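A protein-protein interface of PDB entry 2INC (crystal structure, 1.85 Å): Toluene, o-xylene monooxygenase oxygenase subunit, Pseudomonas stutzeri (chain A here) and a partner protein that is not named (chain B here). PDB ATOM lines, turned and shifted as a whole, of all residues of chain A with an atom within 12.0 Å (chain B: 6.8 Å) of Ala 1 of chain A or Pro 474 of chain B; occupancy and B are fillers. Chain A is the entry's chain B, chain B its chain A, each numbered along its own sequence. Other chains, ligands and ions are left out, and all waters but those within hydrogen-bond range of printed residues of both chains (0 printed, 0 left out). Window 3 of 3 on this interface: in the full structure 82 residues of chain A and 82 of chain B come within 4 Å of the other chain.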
ATOM      1  N   ALA A   1      -3.557  14.582  11.164  1.00  0.00           N
ATOM      2  CA  ALA A   1      -4.996  14.371  10.803  1.00  0.00           C
ATOM      3  C   ALA A   1      -5.889  14.750  11.984  1.00  0.00           C
ATOM      4  O   ALA A   1      -5.528  14.529  13.156  1.00  0.00           O
ATOM      5  CB  ALA A   1      -5.233  12.932  10.396  1.00  0.00           C
ATOM      6  N   LEU A   2      -7.035  15.360  11.664  1.00  0.00           N
ATOM      7  CA  LEU A   2      -8.088  15.709  12.631  1.00  0.00           C
ATOM      8  C   LEU A   2      -8.694  14.440  13.223  1.00  0.00           C
ATOM      9  O   LEU A   2      -9.175  13.559  12.489  1.00  0.00           O
ATOM     10  CB  LEU A   2      -9.202  16.479  11.909  1.00  0.00           C
ATOM     11  CG  LEU A   2      -9.054  17.963  11.584  1.00  0.00           C
ATOM     12  CD1 LEU A   2     -10.203  18.379  10.658  1.00  0.00           C
ATOM     13  CD2 LEU A   2      -9.003  18.827  12.853  1.00  0.00           C
ATOM     14  N   LYS A   3      -8.665  14.339  14.541  1.00  0.00           N
ATOM     15  CA  LYS A   3      -9.197  13.156  15.213  1.00  0.00           C
ATOM     16  C   LYS A   3     -10.725  13.244  15.433  1.00  0.00           C
ATOM     17  O   LYS A   3     -11.255  14.324  15.682  1.00  0.00           O
ATOM     18  CB  LYS A   3      -8.446  12.904  16.541  1.00  0.00           C
ATOM     19  CG  LYS A   3      -7.000  12.398  16.352  1.00  0.00           C
ATOM     20  CD  LYS A   3      -6.959  11.089  15.490  1.00  0.00           C
ATOM     21  CE  LYS A   3      -5.528  10.730  14.978  1.00  0.00           C
ATOM     22  NZ  LYS A   3      -5.047  11.588  13.804  1.00  0.00           N
ATOM     23  N   PRO A   4     -11.437  12.108  15.310  1.00  0.00           N
ATOM     24  CA  PRO A   4     -12.864  12.027  15.650  1.00  0.00           C
ATOM     25  C   PRO A   4     -13.229  12.612  17.002  1.00  0.00           C
ATOM     26  O   PRO A   4     -12.477  12.477  17.983  1.00  0.00           O
ATOM     27  CB  PRO A   4     -13.119  10.519  15.646  1.00  0.00           C
ATOM     28  CG  PRO A   4     -12.207  10.020  14.605  1.00  0.00           C
ATOM     29  CD  PRO A   4     -10.946  10.820  14.776  1.00  0.00           C
ATOM     30  N   LEU A   5     -14.384  13.274  17.057  1.00  0.00           N
ATOM     31  CA  LEU A   5     -14.853  13.877  18.306  1.00  0.00           C
ATOM     32  C   LEU A   5     -15.960  13.001  18.884  1.00  0.00           C
ATOM     33  O   LEU A   5     -16.466  12.109  18.200  1.00  0.00           O
ATOM     34  CB  LEU A   5     -15.344  15.322  18.062  1.00  0.00           C
ATOM     35  CG  LEU A   5     -14.356  16.343  17.482  1.00  0.00           C
ATOM     36  CD1 LEU A   5     -15.070  17.598  17.030  1.00  0.00           C
ATOM     37  CD2 LEU A   5     -13.285  16.694  18.517  1.00  0.00           C
ATOM     38  N   ARG B 152     -14.009  12.338  11.527  1.00  0.00           N
ATOM     39  CA  ARG B 152     -14.409  13.728  11.506  1.00  0.00           C
ATOM     40  C   ARG B 152     -15.280  14.055  10.308  1.00  0.00           C
ATOM     41  O   ARG B 152     -15.974  15.061  10.311  1.00  0.00           O
ATOM     42  CB  ARG B 152     -13.171  14.610  11.454  1.00  0.00           C
ATOM     43  CG  ARG B 152     -13.459  16.010  11.934  1.00  0.00           C
ATOM     44  CD  ARG B 152     -13.535  16.070  13.439  1.00  0.00           C
ATOM     45  NE  ARG B 152     -13.247  17.426  13.824  1.00  0.00           N
ATOM     46  CZ  ARG B 152     -12.283  17.818  14.636  1.00  0.00           C
ATOM     47  NH1 ARG B 152     -11.478  16.963  15.264  1.00  0.00           N
ATOM     48  NH2 ARG B 152     -12.167  19.110  14.840  1.00  0.00           N
ATOM     49  N   LEU B 472     -11.186  22.869   5.281  1.00  0.00           N
ATOM     50  CA  LEU B 472     -10.738  21.494   5.126  1.00  0.00           C
ATOM     51  C   LEU B 472      -9.315  21.273   5.597  1.00  0.00           C
ATOM     52  O   LEU B 472      -8.402  21.992   5.147  1.00  0.00           O
ATOM     53  CB  LEU B 472     -10.748  21.144   3.652  1.00  0.00           C
ATOM     54  CG  LEU B 472     -12.136  21.089   3.037  1.00  0.00           C
ATOM     55  CD1 LEU B 472     -12.023  21.185   1.535  1.00  0.00           C
ATOM     56  CD2 LEU B 472     -12.797  19.791   3.462  1.00  0.00           C
ATOM     57  N   GLU B 473      -9.132  20.226   6.401  1.00  0.00           N
ATOM     58  CA  GLU B 473      -7.842  19.789   6.937  1.00  0.00           C
ATOM     59  C   GLU B 473      -7.685  18.274   6.761  1.00  0.00           C
ATOM     60  O   GLU B 473      -8.665  17.574   6.490  1.00  0.00           O
ATOM     61  CB  GLU B 473      -7.763  20.147   8.416  1.00  0.00           C
ATOM     62  CG  GLU B 473      -7.887  21.639   8.638  1.00  0.00           C
ATOM     63  CD  GLU B 473      -8.248  21.987  10.066  1.00  0.00           C
ATOM     64  OE1 GLU B 473      -9.456  22.242  10.325  1.00  0.00           O
ATOM     65  OE2 GLU B 473      -7.335  21.978  10.930  1.00  0.00           O
ATOM     66  N   PRO B 474      -6.441  17.757   6.854  1.00  0.00           N
ATOM     67  CA  PRO B 474      -6.284  16.300   6.738  1.00  0.00           C
ATOM     68  C   PRO B 474      -7.158  15.560   7.748  1.00  0.00           C
ATOM     69  O   PRO B 474      -7.278  15.980   8.902  1.00  0.00           O
ATOM     70  CB  PRO B 474      -4.781  16.079   7.032  1.00  0.00           C
ATOM     71  CG  PRO B 474      -4.133  17.383   6.627  1.00  0.00           C
ATOM     72  CD  PRO B 474      -5.141  18.452   6.982  1.00  0.00           C
ATOM     73  N   GLY B 475      -7.766  14.463   7.311  1.00  0.00           N
ATOM     74  CA  GLY B 475      -8.714  13.786   8.164  1.00  0.00           C
ATOM     75  C   GLY B 475     -10.109  13.896   7.579  1.00  0.00           C
ATOM     76  O   GLY B 475     -10.906  12.943   7.694  1.00  0.00           O
ATOM     77  N   VAL B 476     -10.418  15.054   6.991  1.00  0.00           N
ATOM     78  CA  VAL B 476     -11.644  15.178   6.202  1.00  0.00           C
ATOM     79  C   VAL B 476     -11.436  15.342   4.705  1.00  0.00           C
ATOM     80  O   VAL B 476     -12.270  14.911   3.937  1.00  0.00           O
ATOM     81  CB  VAL B 476     -12.796  16.083   6.833  1.00  0.00           C
ATOM     82  CG1 VAL B 476     -12.516  16.476   8.277  1.00  0.00           C
ATOM     83  CG2 VAL B 476     -13.167  17.244   6.020  1.00  0.00           C
ATOM     84  N   MET B 477     -10.329  15.950   4.286  1.00  0.00           N
ATOM     85  CA  MET B 477     -10.020  16.092   2.846  1.00  0.00           C
ATOM     86  C   MET B 477     -10.143  14.760   2.118  1.00  0.00           C
ATOM     87  O   MET B 477      -9.618  13.745   2.591  1.00  0.00           O
ATOM     88  CB  MET B 477      -8.604  16.640   2.626  1.00  0.00           C
ATOM     89  CG  MET B 477      -8.449  18.106   2.962  1.00  0.00           C
ATOM     90  SD  MET B 477      -6.704  18.540   3.287  1.00  0.00           S
ATOM     91  CE  MET B 477      -5.994  18.136   1.686  1.00  0.00           C
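The backbone carbonyl oxygen (O) of Lys 3 of chain A is in hydrogen-bond range of the guanidinium group (NH1) of Arg 152 of chain B (2.7 Å). The backbone carbonyl oxygen (O) of Pro 474 of chain B is in hydrogen-bond range of the backbone NH (N) of Leu 2 of chain A (2.8 Å).
The backbone carbonyl oxygen (O) of Ala 1 of chain A lies within hydrogen-bond range of the side-chain amino group (NZ) of Lys 3 of chain A (3.0 Å).
Ala 1 of chain A touches Pro 474 of chain B. Leu 2 of chain A touches Arg 152 of chain B (CD2 to NH2, 3.7 Å). Leu 2 of chain A touches Glu 473 of chain B (CD1 to CB, 3.8 Å). CD1 of Leu 2 of chain A touches CG1 of Val 476 of chain B, at 3.8 Å. Arg 152 of chain B touches Leu 5 of chain A.
Ala 1 of chain A touches just one residue of chain B: Pro 474 (3.4 Å). Pro 474 of chain B touches just these residues of chain A: Ala 1 and Leu 2. No residue of chain A comes within 4 Å of Gly 475 of chain B. Of chain A, only Leu 2 comes within 4 Å of Val 476 of chain B. No residue of chain A comes within 4 Å of Met 477 of chain B. Of the printed residues of chain B, Leu 5 of chain A touches Arg 152 (3.7 Å). Printed residues of chain B within 4 Å of Leu 2 of chain A: Arg 152 (3.7 Å), Glu 473 (3.8 Å), Pro 474 (2.8 Å) and Val 476 (3.8 Å). Pro 4 of chain A touches none of the printed residues of chain B. Leu 472 of chain B touches none of the printed residues of chain A. The nearest residue of chain B that does not touch Ala 1 of chain A is Gly 475 of chain B (4.2 Å).
Hydrophobic or aromatic side chains of chain B that line the printed part of chain A: Val 476. Along chain B the printed residues that touch a printed residue of chain A span positions 152 to 476. Of the 5 printed residues of chain A, 4 touch a printed residue of chain B. Printed residues of chain A that touch a printed residue of chain B: Ala 1, Leu 2, Lys 3 and Leu 5. Among the printed residues, no Asp or Glu carboxylate lies within 4 Å of a Lys or Arg side-chain nitrogen of the other chain.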
